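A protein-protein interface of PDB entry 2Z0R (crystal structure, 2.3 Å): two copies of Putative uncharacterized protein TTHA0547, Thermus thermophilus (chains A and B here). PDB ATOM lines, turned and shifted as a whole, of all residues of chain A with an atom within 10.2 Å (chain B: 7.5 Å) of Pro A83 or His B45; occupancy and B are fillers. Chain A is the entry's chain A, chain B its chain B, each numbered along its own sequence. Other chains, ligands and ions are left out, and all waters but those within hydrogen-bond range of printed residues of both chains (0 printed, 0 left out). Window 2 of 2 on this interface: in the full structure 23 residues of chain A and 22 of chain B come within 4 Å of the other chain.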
ATOM      1  N   TRP A  33     -34.078  18.125   3.819  1.00  0.00           N
ATOM      2  CA  TRP A  33     -32.972  17.274   3.396  1.00  0.00           C
ATOM      3  C   TRP A  33     -33.444  15.919   2.901  1.00  0.00           C
ATOM      4  O   TRP A  33     -34.442  15.377   3.388  1.00  0.00           O
ATOM      5  CB  TRP A  33     -31.964  17.103   4.533  1.00  0.00           C
ATOM      6  CG  TRP A  33     -31.104  18.307   4.713  1.00  0.00           C
ATOM      7  CD1 TRP A  33     -29.904  18.543   4.124  1.00  0.00           C
ATOM      8  CD2 TRP A  33     -31.409  19.478   5.483  1.00  0.00           C
ATOM      9  NE1 TRP A  33     -29.434  19.784   4.472  1.00  0.00           N
ATOM     10  CE2 TRP A  33     -30.341  20.383   5.306  1.00  0.00           C
ATOM     11  CE3 TRP A  33     -32.483  19.851   6.304  1.00  0.00           C
ATOM     12  CZ2 TRP A  33     -30.313  21.645   5.923  1.00  0.00           C
ATOM     13  CZ3 TRP A  33     -32.455  21.099   6.915  1.00  0.00           C
ATOM     14  CH2 TRP A  33     -31.376  21.982   6.721  1.00  0.00           C
ATOM     15  N   GLU A  37     -27.929  12.154   6.710  1.00  0.00           N
ATOM     16  CA  GLU A  37     -26.532  12.514   6.902  1.00  0.00           C
ATOM     17  C   GLU A  37     -26.320  14.012   6.767  1.00  0.00           C
ATOM     18  O   GLU A  37     -25.674  14.641   7.603  1.00  0.00           O
ATOM     19  CB  GLU A  37     -25.657  11.770   5.883  1.00  0.00           C
ATOM     20  CG  GLU A  37     -24.285  12.393   5.642  1.00  0.00           C
ATOM     21  CD  GLU A  37     -23.440  12.460   6.898  1.00  0.00           C
ATOM     22  OE1 GLU A  37     -22.360  13.087   6.853  1.00  0.00           O
ATOM     23  OE2 GLU A  37     -23.854  11.882   7.930  1.00  0.00           O
ATOM     24  N   LEU A  38     -26.858  14.582   5.701  1.00  0.00           N
ATOM     25  CA  LEU A  38     -26.723  16.009   5.476  1.00  0.00           C
ATOM     26  C   LEU A  38     -27.484  16.800   6.531  1.00  0.00           C
ATOM     27  O   LEU A  38     -26.996  17.819   7.022  1.00  0.00           O
ATOM     28  CB  LEU A  38     -27.226  16.367   4.080  1.00  0.00           C
ATOM     29  CG  LEU A  38     -26.368  15.827   2.936  1.00  0.00           C
ATOM     30  CD1 LEU A  38     -26.947  16.278   1.597  1.00  0.00           C
ATOM     31  CD2 LEU A  38     -24.945  16.323   3.100  1.00  0.00           C
ATOM     32  N   ALA A  39     -28.673  16.325   6.885  1.00  0.00           N
ATOM     33  CA  ALA A  39     -29.492  16.998   7.886  1.00  0.00           C
ATOM     34  C   ALA A  39     -28.802  17.002   9.245  1.00  0.00           C
ATOM     35  O   ALA A  39     -28.729  18.040   9.911  1.00  0.00           O
ATOM     36  CB  ALA A  39     -30.852  16.325   7.986  1.00  0.00           C
ATOM     37  N   ALA A  41     -25.644  16.577   9.757  1.00  0.00           N
ATOM     38  CA  ALA A  41     -24.372  17.291   9.663  1.00  0.00           C
ATOM     39  C   ALA A  41     -24.661  18.785   9.800  1.00  0.00           C
ATOM     40  O   ALA A  41     -23.914  19.520  10.447  1.00  0.00           O
ATOM     41  CB  ALA A  41     -23.682  16.991   8.333  1.00  0.00           C
ATOM     42  N   PHE A  42     -25.759  19.234   9.205  1.00  0.00           N
ATOM     43  CA  PHE A  42     -26.128  20.641   9.298  1.00  0.00           C
ATOM     44  C   PHE A  42     -26.472  20.969  10.750  1.00  0.00           C
ATOM     45  O   PHE A  42     -26.056  21.995  11.291  1.00  0.00           O
ATOM     46  CB  PHE A  42     -27.347  20.938   8.429  1.00  0.00           C
ATOM     47  CG  PHE A  42     -27.882  22.337   8.599  1.00  0.00           C
ATOM     48  CD1 PHE A  42     -27.401  23.391   7.811  1.00  0.00           C
ATOM     49  CD2 PHE A  42     -28.858  22.611   9.551  1.00  0.00           C
ATOM     50  CE1 PHE A  42     -27.890  24.691   7.970  1.00  0.00           C
ATOM     51  CE2 PHE A  42     -29.349  23.914   9.716  1.00  0.00           C
ATOM     52  CZ  PHE A  42     -28.863  24.952   8.923  1.00  0.00           C
ATOM     53  N   LEU A  43     -27.246  20.095  11.378  1.00  0.00           N
ATOM     54  CA  LEU A  43     -27.647  20.327  12.753  1.00  0.00           C
ATOM     55  C   LEU A  43     -26.426  20.389  13.658  1.00  0.00           C
ATOM     56  O   LEU A  43     -26.345  21.247  14.540  1.00  0.00           O
ATOM     57  CB  LEU A  43     -28.603  19.226  13.225  1.00  0.00           C
ATOM     58  CG  LEU A  43     -29.089  19.349  14.672  1.00  0.00           C
ATOM     59  CD1 LEU A  43     -29.759  20.702  14.896  1.00  0.00           C
ATOM     60  CD2 LEU A  43     -30.059  18.219  14.972  1.00  0.00           C
ATOM     61  N   ALA A  44     -25.467  19.497  13.417  1.00  0.00           N
ATOM     62  CA  ALA A  44     -24.255  19.444  14.226  1.00  0.00           C
ATOM     63  C   ALA A  44     -23.484  20.746  14.197  1.00  0.00           C
ATOM     64  O   ALA A  44     -22.789  21.067  15.156  1.00  0.00           O
ATOM     65  CB  ALA A  44     -23.365  18.314  13.763  1.00  0.00           C
ATOM     66  N   HIS A  45     -23.610  21.486  13.098  1.00  0.00           N
ATOM     67  CA  HIS A  45     -22.929  22.771  12.932  1.00  0.00           C
ATOM     68  C   HIS A  45     -23.798  23.951  13.342  1.00  0.00           C
ATOM     69  O   HIS A  45     -23.368  25.096  13.280  1.00  0.00           O
ATOM     70  CB  HIS A  45     -22.486  22.949  11.475  1.00  0.00           C
ATOM     71  CG  HIS A  45     -21.484  21.933  11.031  1.00  0.00           C
ATOM     72  ND1 HIS A  45     -21.630  21.199   9.874  1.00  0.00           N
ATOM     73  CD2 HIS A  45     -20.345  21.494  11.616  1.00  0.00           C
ATOM     74  CE1 HIS A  45     -20.626  20.346   9.768  1.00  0.00           C
ATOM     75  NE2 HIS A  45     -19.832  20.506  10.812  1.00  0.00           N
ATOM     76  N   HIS A  46     -25.027  23.665  13.751  1.00  0.00           N
ATOM     77  CA  HIS A  46     -25.948  24.703  14.194  1.00  0.00           C
ATOM     78  C   HIS A  46     -26.508  24.342  15.563  1.00  0.00           C
ATOM     79  O   HIS A  46     -27.653  23.907  15.707  1.00  0.00           O
ATOM     80  CB  HIS A  46     -27.063  24.896  13.169  1.00  0.00           C
ATOM     81  CG  HIS A  46     -26.566  25.437  11.869  1.00  0.00           C
ATOM     82  ND1 HIS A  46     -25.880  24.662  10.960  1.00  0.00           N
ATOM     83  CD2 HIS A  46     -26.542  26.700  11.382  1.00  0.00           C
ATOM     84  CE1 HIS A  46     -25.446  25.426   9.974  1.00  0.00           C
ATOM     85  NE2 HIS A  46     -25.833  26.667  10.206  1.00  0.00           N
ATOM     86  N   PRO A  47     -25.673  24.501  16.593  1.00  0.00           N
ATOM     87  CA  PRO A  47     -26.020  24.212  17.982  1.00  0.00           C
ATOM     88  C   PRO A  47     -26.689  25.427  18.601  1.00  0.00           C
ATOM     89  O   PRO A  47     -26.662  26.514  18.026  1.00  0.00           O
ATOM     90  CB  PRO A  47     -24.659  23.943  18.635  1.00  0.00           C
ATOM     91  CG  PRO A  47     -23.691  23.792  17.458  1.00  0.00           C
ATOM     92  CD  PRO A  47     -24.229  24.752  16.469  1.00  0.00           C
ATOM     93  N   MET A  78     -34.937  25.185   1.013  1.00  0.00           N
ATOM     94  CA  MET A  78     -33.653  24.838   0.439  1.00  0.00           C
ATOM     95  C   MET A  78     -33.583  23.325   0.520  1.00  0.00           C
ATOM     96  O   MET A  78     -33.900  22.741   1.562  1.00  0.00           O
ATOM     97  CB  MET A  78     -32.527  25.438   1.270  1.00  0.00           C
ATOM     98  CG  MET A  78     -31.424  26.075   0.460  1.00  0.00           C
ATOM     99  SD  MET A  78     -31.636  27.977   0.372  1.00  0.00           S
ATOM    100  CE  MET A  78     -30.838  28.435   2.069  1.00  0.00           C
ATOM    101  N   VAL A  79     -33.180  22.685  -0.572  1.00  0.00           N
ATOM    102  CA  VAL A  79     -33.080  21.231  -0.587  1.00  0.00           C
ATOM    103  C   VAL A  79     -31.629  20.794  -0.421  1.00  0.00           C
ATOM    104  O   VAL A  79     -30.757  21.193  -1.193  1.00  0.00           O
ATOM    105  CB  VAL A  79     -33.650  20.656  -1.893  1.00  0.00           C
ATOM    106  CG1 VAL A  79     -33.627  19.140  -1.854  1.00  0.00           C
ATOM    107  CG2 VAL A  79     -35.066  21.157  -2.097  1.00  0.00           C
ATOM    108  N   ASP A  80     -31.380  19.990   0.608  1.00  0.00           N
ATOM    109  CA  ASP A  80     -30.044  19.484   0.909  1.00  0.00           C
ATOM    110  C   ASP A  80     -28.973  20.574   0.995  1.00  0.00           C
ATOM    111  O   ASP A  80     -27.902  20.455   0.401  1.00  0.00           O
ATOM    112  CB  ASP A  80     -29.628  18.428  -0.123  1.00  0.00           C
ATOM    113  CG  ASP A  80     -30.289  17.073   0.122  1.00  0.00           C
ATOM    114  OD1 ASP A  80     -30.273  16.612   1.282  1.00  0.00           O
ATOM    115  OD2 ASP A  80     -30.810  16.463  -0.841  1.00  0.00           O
ATOM    116  N   TYR A  81     -29.258  21.626   1.754  1.00  0.00           N
ATOM    117  CA  TYR A  81     -28.317  22.728   1.914  1.00  0.00           C
ATOM    118  C   TYR A  81     -27.046  22.273   2.641  1.00  0.00           C
ATOM    119  O   TYR A  81     -27.097  21.402   3.515  1.00  0.00           O
ATOM    120  CB  TYR A  81     -28.979  23.857   2.705  1.00  0.00           C
ATOM    121  CG  TYR A  81     -28.117  25.087   2.875  1.00  0.00           C
ATOM    122  CD1 TYR A  81     -28.005  26.030   1.854  1.00  0.00           C
ATOM    123  CD2 TYR A  81     -27.407  25.307   4.057  1.00  0.00           C
ATOM    124  CE1 TYR A  81     -27.213  27.159   2.003  1.00  0.00           C
ATOM    125  CE2 TYR A  81     -26.607  26.437   4.217  1.00  0.00           C
ATOM    126  CZ  TYR A  81     -26.519  27.357   3.184  1.00  0.00           C
ATOM    127  OH  TYR A  81     -25.737  28.475   3.330  1.00  0.00           O
ATOM    128  N   ARG A  82     -25.912  22.869   2.274  1.00  0.00           N
ATOM    129  CA  ARG A  82     -24.618  22.566   2.887  1.00  0.00           C
ATOM    130  C   ARG A  82     -23.543  23.468   2.289  1.00  0.00           C
ATOM    131  O   ARG A  82     -23.680  23.926   1.160  1.00  0.00           O
ATOM    132  CB  ARG A  82     -24.240  21.102   2.661  1.00  0.00           C
ATOM    133  CG  ARG A  82     -24.145  20.707   1.207  1.00  0.00           C
ATOM    134  CD  ARG A  82     -24.094  19.200   1.068  1.00  0.00           C
ATOM    135  NE  ARG A  82     -24.362  18.774  -0.303  1.00  0.00           N
ATOM    136  CZ  ARG A  82     -23.462  18.780  -1.278  1.00  0.00           C
ATOM    137  NH1 ARG A  82     -22.220  19.185  -1.040  1.00  0.00           N
ATOM    138  NH2 ARG A  82     -23.806  18.386  -2.495  1.00  0.00           N
ATOM    139  N   PRO A  83     -22.465  23.741   3.044  1.00  0.00           N
ATOM    140  CA  PRO A  83     -21.381  24.597   2.552  1.00  0.00           C
ATOM    141  C   PRO A  83     -20.642  23.924   1.412  1.00  0.00           C
ATOM    142  O   PRO A  83     -20.752  22.714   1.223  1.00  0.00           O
ATOM    143  CB  PRO A  83     -20.472  24.761   3.771  1.00  0.00           C
ATOM    144  CG  PRO A  83     -21.366  24.453   4.946  1.00  0.00           C
ATOM    145  CD  PRO A  83     -22.191  23.306   4.423  1.00  0.00           C
ATOM    146  N   GLY A  84     -19.893  24.718   0.653  1.00  0.00           N
ATOM    147  CA  GLY A  84     -19.107  24.194  -0.450  1.00  0.00           C
ATOM    148  C   GLY A  84     -19.850  23.713  -1.681  1.00  0.00           C
ATOM    149  O   GLY A  84     -19.382  22.809  -2.371  1.00  0.00           O
ATOM    150  N   THR A  85     -21.001  24.302  -1.972  1.00  0.00           N
ATOM    151  CA  THR A  85     -21.760  23.895  -3.145  1.00  0.00           C
ATOM    152  C   THR A  85     -21.632  25.018  -4.161  1.00  0.00           C
ATOM    153  O   THR A  85     -21.334  26.152  -3.791  1.00  0.00           O
ATOM    154  CB  THR A  85     -23.257  23.688  -2.809  1.00  0.00           C
ATOM    155  OG1 THR A  85     -23.378  22.910  -1.614  1.00  0.00           O
ATOM    156  CG2 THR A  85     -23.956  22.949  -3.940  1.00  0.00           C
ATOM    157  N   HIS A  86     -21.837  24.709  -5.439  1.00  0.00           N
ATOM    158  CA  HIS A  86     -21.755  25.743  -6.464  1.00  0.00           C
ATOM    159  C   HIS A  86     -22.977  26.642  -6.312  1.00  0.00           C
ATOM    160  O   HIS A  86     -22.852  27.859  -6.175  1.00  0.00           O
ATOM    161  CB  HIS A  86     -21.728  25.126  -7.867  1.00  0.00           C
ATOM    162  CG  HIS A  86     -21.634  26.139  -8.967  1.00  0.00           C
ATOM    163  ND1 HIS A  86     -20.593  27.035  -9.067  1.00  0.00           N
ATOM    164  CD2 HIS A  86     -22.462  26.408 -10.006  1.00  0.00           C
ATOM    165  CE1 HIS A  86     -20.782  27.815 -10.116  1.00  0.00           C
ATOM    166  NE2 HIS A  86     -21.909  27.456 -10.703  1.00  0.00           N
ATOM    167  N   ARG A  87     -24.156  26.030  -6.335  1.00  0.00           N
ATOM    168  CA  ARG A  87     -25.418  26.749  -6.177  1.00  0.00           C
ATOM    169  C   ARG A  87     -26.328  25.932  -5.267  1.00  0.00           C
ATOM    170  O   ARG A  87     -26.099  24.737  -5.051  1.00  0.00           O
ATOM    171  CB  ARG A  87     -26.107  26.955  -7.528  1.00  0.00           C
ATOM    172  CG  ARG A  87     -25.292  27.750  -8.547  1.00  0.00           C
ATOM    173  CD  ARG A  87     -25.140  29.221  -8.169  1.00  0.00           C
ATOM    174  NE  ARG A  87     -24.238  29.916  -9.086  1.00  0.00           N
ATOM    175  CZ  ARG A  87     -23.921  31.207  -9.003  1.00  0.00           C
ATOM    176  NH1 ARG A  87     -24.437  31.961  -8.040  1.00  0.00           N
ATOM    177  NH2 ARG A  87     -23.081  31.745  -9.881  1.00  0.00           N
ATOM    178  N   ALA A  88     -27.358  26.578  -4.733  1.00  0.00           N
ATOM    179  CA  ALA A  88     -28.294  25.899  -3.847  1.00  0.00           C
ATOM    180  C   ALA A  88     -29.517  25.445  -4.622  1.00  0.00           C
ATOM    181  O   ALA A  88     -29.834  25.998  -5.671  1.00  0.00           O
ATOM    182  CB  ALA A  88     -28.710  26.824  -2.707  1.00  0.00           C
ATOM    183  N   ALA B  39     -17.163  36.859  11.387  1.00  0.00           N
ATOM    184  CA  ALA B  39     -18.323  37.021  10.526  1.00  0.00           C
ATOM    185  C   ALA B  39     -18.103  36.335   9.173  1.00  0.00           C
ATOM    186  O   ALA B  39     -19.000  35.665   8.653  1.00  0.00           O
ATOM    187  CB  ALA B  39     -18.638  38.495  10.337  1.00  0.00           C
ATOM    188  N   GLU B  40     -16.912  36.481   8.604  1.00  0.00           N
ATOM    189  CA  GLU B  40     -16.633  35.842   7.318  1.00  0.00           C
ATOM    190  C   GLU B  40     -16.594  34.322   7.474  1.00  0.00           C
ATOM    191  O   GLU B  40     -16.968  33.580   6.562  1.00  0.00           O
ATOM    192  CB  GLU B  40     -15.316  36.365   6.738  1.00  0.00           C
ATOM    193  CG  GLU B  40     -15.381  37.830   6.334  1.00  0.00           C
ATOM    194  CD  GLU B  40     -14.070  38.324   5.761  1.00  0.00           C
ATOM    195  OE1 GLU B  40     -13.018  38.071   6.385  1.00  0.00           O
ATOM    196  OE2 GLU B  40     -14.089  38.972   4.691  1.00  0.00           O
ATOM    197  N   ALA B  41     -16.147  33.856   8.634  1.00  0.00           N
ATOM    198  CA  ALA B  41     -16.117  32.425   8.899  1.00  0.00           C
ATOM    199  C   ALA B  41     -17.560  31.931   8.824  1.00  0.00           C
ATOM    200  O   ALA B  41     -17.858  30.949   8.146  1.00  0.00           O
ATOM    201  CB  ALA B  41     -15.534  32.153  10.288  1.00  0.00           C
ATOM    202  N   PHE B  42     -18.463  32.624   9.515  1.00  0.00           N
ATOM    203  CA  PHE B  42     -19.869  32.242   9.489  1.00  0.00           C
ATOM    204  C   PHE B  42     -20.391  32.352   8.057  1.00  0.00           C
ATOM    205  O   PHE B  42     -21.149  31.501   7.586  1.00  0.00           O
ATOM    206  CB  PHE B  42     -20.698  33.149  10.401  1.00  0.00           C
ATOM    207  CG  PHE B  42     -22.177  32.901  10.307  1.00  0.00           C
ATOM    208  CD1 PHE B  42     -22.779  31.908  11.063  1.00  0.00           C
ATOM    209  CD2 PHE B  42     -22.964  33.642   9.429  1.00  0.00           C
ATOM    210  CE1 PHE B  42     -24.148  31.653  10.950  1.00  0.00           C
ATOM    211  CE2 PHE B  42     -24.336  33.391   9.307  1.00  0.00           C
ATOM    212  CZ  PHE B  42     -24.928  32.395  10.071  1.00  0.00           C
ATOM    213  N   LEU B  43     -19.992  33.413   7.367  1.00  0.00           N
ATOM    214  CA  LEU B  43     -20.431  33.625   5.988  1.00  0.00           C
ATOM    215  C   LEU B  43     -19.973  32.451   5.120  1.00  0.00           C
ATOM    216  O   LEU B  43     -20.718  31.971   4.270  1.00  0.00           O
ATOM    217  CB  LEU B  43     -19.838  34.923   5.444  1.00  0.00           C
ATOM    218  CG  LEU B  43     -20.656  35.819   4.512  1.00  0.00           C
ATOM    219  CD1 LEU B  43     -19.697  36.790   3.834  1.00  0.00           C
ATOM    220  CD2 LEU B  43     -21.417  35.000   3.481  1.00  0.00           C
ATOM    221  N   ALA B  44     -18.746  31.988   5.352  1.00  0.00           N
ATOM    222  CA  ALA B  44     -18.194  30.866   4.597  1.00  0.00           C
ATOM    223  C   ALA B  44     -19.023  29.588   4.763  1.00  0.00           C
ATOM    224  O   ALA B  44     -19.048  28.754   3.870  1.00  0.00           O
ATOM    225  CB  ALA B  44     -16.746  30.607   5.024  1.00  0.00           C
ATOM    226  N   HIS B  45     -19.703  29.433   5.896  1.00  0.00           N
ATOM    227  CA  HIS B  45     -20.525  28.245   6.126  1.00  0.00           C
ATOM    228  C   HIS B  45     -21.996  28.434   5.737  1.00  0.00           C
ATOM    229  O   HIS B  45     -22.814  27.538   5.943  1.00  0.00           O
ATOM    230  CB  HIS B  45     -20.428  27.806   7.591  1.00  0.00           C
ATOM    231  CG  HIS B  45     -19.071  27.308   7.982  1.00  0.00           C
ATOM    232  ND1 HIS B  45     -18.479  27.623   9.187  1.00  0.00           N
ATOM    233  CD2 HIS B  45     -18.179  26.535   7.315  1.00  0.00           C
ATOM    234  CE1 HIS B  45     -17.279  27.070   9.244  1.00  0.00           C
ATOM    235  NE2 HIS B  45     -17.073  26.405   8.121  1.00  0.00           N
ATOM    236  N   HIS B  46     -22.335  29.594   5.174  1.00  0.00           N
ATOM    237  CA  HIS B  46     -23.712  29.849   4.747  1.00  0.00           C
ATOM    238  C   HIS B  46     -23.780  30.606   3.424  1.00  0.00           C
ATOM    239  O   HIS B  46     -24.153  31.774   3.382  1.00  0.00           O
ATOM    240  CB  HIS B  46     -24.479  30.619   5.823  1.00  0.00           C
ATOM    241  CG  HIS B  46     -24.512  29.912   7.137  1.00  0.00           C
ATOM    242  ND1 HIS B  46     -23.435  29.907   8.001  1.00  0.00           N
ATOM    243  CD2 HIS B  46     -25.428  29.071   7.672  1.00  0.00           C
ATOM    244  CE1 HIS B  46     -23.682  29.081   9.001  1.00  0.00           C
ATOM    245  NE2 HIS B  46     -24.884  28.560   8.824  1.00  0.00           N
ATOM    246  N   PRO B  47     -23.415  29.936   2.319  1.00  0.00           N
ATOM    247  CA  PRO B  47     -23.435  30.545   0.990  1.00  0.00           C
ATOM    248  C   PRO B  47     -24.836  30.528   0.397  1.00  0.00           C
ATOM    249  O   PRO B  47     -25.777  30.017   1.007  1.00  0.00           O
ATOM    250  CB  PRO B  47     -22.480  29.660   0.203  1.00  0.00           C
ATOM    251  CG  PRO B  47     -22.801  28.309   0.748  1.00  0.00           C
ATOM    252  CD  PRO B  47     -22.871  28.565   2.250  1.00  0.00           C
ATOM    253  N   HIS B  48     -24.960  31.109  -0.790  1.00  0.00           N
ATOM    254  CA  HIS B  48     -26.215  31.150  -1.517  1.00  0.00           C
ATOM    255  C   HIS B  48     -27.364  31.882  -0.844  1.00  0.00           C
ATOM    256  O   HIS B  48     -28.523  31.687  -1.212  1.00  0.00           O
ATOM    257  CB  HIS B  48     -26.612  29.724  -1.859  1.00  0.00           C
ATOM    258  CG  HIS B  48     -25.484  28.930  -2.431  1.00  0.00           C
ATOM    259  ND1 HIS B  48     -25.261  27.607  -2.110  1.00  0.00           N
ATOM    260  CD2 HIS B  48     -24.483  29.289  -3.270  1.00  0.00           C
ATOM    261  CE1 HIS B  48     -24.169  27.187  -2.723  1.00  0.00           C
ATOM    262  NE2 HIS B  48     -23.678  28.188  -3.433  1.00  0.00           N
ATOM    263  N   LEU B  49     -27.039  32.725   0.131  1.00  0.00           N
ATOM    264  CA  LEU B  49     -28.036  33.522   0.835  1.00  0.00           C
ATOM    265  C   LEU B  49     -27.926  34.976   0.392  1.00  0.00           C
ATOM    266  O   LEU B  49     -28.612  35.844   0.929  1.00  0.00           O
ATOM    267  CB  LEU B  49     -27.834  33.427   2.353  1.00  0.00           C
ATOM    268  CG  LEU B  49     -28.111  32.051   2.969  1.00  0.00           C
ATOM    269  CD1 LEU B  49     -27.762  32.066   4.454  1.00  0.00           C
ATOM    270  CD2 LEU B  49     -29.587  31.669   2.755  1.00  0.00           C
ATOM    271  N   ARG B  82     -21.213  30.672  16.373  1.00  0.00           N
ATOM    272  CA  ARG B  82     -20.366  29.738  15.646  1.00  0.00           C
ATOM    273  C   ARG B  82     -20.510  28.355  16.263  1.00  0.00           C
ATOM    274  O   ARG B  82     -21.017  28.213  17.376  1.00  0.00           O
ATOM    275  CB  ARG B  82     -18.900  30.169  15.697  1.00  0.00           C
ATOM    276  CG  ARG B  82     -18.299  30.140  17.081  1.00  0.00           C
ATOM    277  CD  ARG B  82     -16.784  30.191  17.017  1.00  0.00           C
ATOM    278  NE  ARG B  82     -16.204  30.182  18.356  1.00  0.00           N
ATOM    279  CZ  ARG B  82     -16.189  31.233  19.172  1.00  0.00           C
ATOM    280  NH1 ARG B  82     -16.719  32.387  18.781  1.00  0.00           N
ATOM    281  NH2 ARG B  82     -15.664  31.121  20.386  1.00  0.00           N
ATOM    282  N   PRO B  83     -20.104  27.311  15.528  1.00  0.00           N
ATOM    283  CA  PRO B  83     -20.216  25.966  16.100  1.00  0.00           C
ATOM    284  C   PRO B  83     -19.341  25.974  17.361  1.00  0.00           C
ATOM    285  O   PRO B  83     -18.142  25.684  17.295  1.00  0.00           O
ATOM    286  CB  PRO B  83     -19.646  25.077  14.998  1.00  0.00           C
ATOM    287  CG  PRO B  83     -19.954  25.850  13.733  1.00  0.00           C
ATOM    288  CD  PRO B  83     -19.620  27.263  14.135  1.00  0.00           C
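NE2 of His A46 lies within hydrogen-bond range of NE2 of His B46, at 2.5 Å.
OH of Tyr A81 sits at hydrogen-bond distance from O of Pro B47 (2.8 Å).
The backbone carbonyl oxygen of Thr A85 sits at hydrogen-bond distance from a ring nitrogen (NE2) of His B48.
A ring nitrogen (NE2) of His B48 is in hydrogen-bond range of the backbone carbonyl oxygen of His A86 (2.9 Å).
The backbone carbonyl oxygen (O) of Tyr A81 is in hydrogen-bond range of the indole nitrogen (NE1) of Trp A33, at 3.0 Å.
The backbone carbonyl oxygen (O) of Ala A41 sits at hydrogen-bond distance from a ring nitrogen (ND1) of His A45 (2.9 Å).
O of Phe A42 lies within hydrogen-bond range of ND1 of His A46.
The side-chain hydroxyl (OG1) of Thr A85 lies within hydrogen-bond range of the backbone carbonyl oxygen (O) of Arg A82, 3.0 Å away.
The backbone carbonyl oxygen of Phe B42 is in hydrogen-bond range of a ring nitrogen (ND1) of His B46, 2.8 Å away.
Among the printed residues, merely in contact across the chains: His A45 with Pro B83, Met A78 with Leu B49, Tyr A81 with His B46, Pro A83 with His B45, Arg A87 with His B48 and Ala A88 with His B48.
Printed residues of chain B within 4 Å of Pro A83: His B45.
Of chain A, only Pro A83 (3.6 Å) comes within 4 Å of His B45.
No residue of chain A comes within 4 Å of Ala B44.
His B46 touches just these residues of chain A: His A46 and Tyr A81.
Of the printed residues of chain A, Pro B47 touches Tyr A81.
Of the printed residues of chain A, Leu B49 touches Met A78.
Ala A39 touches none of the printed residues of chain B.
Gly A84 touches none of the printed residues of chain B.
The nearest residue of chain A that does not touch His B45 is Tyr A81 (4.03 Å).
Among the printed residues, 10 pairs touch across the chains.
His A45 touches Pro B83, and with the chains exchanged Pro A83 touches His B45.
His A46 touches its own counterpart, His B46.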
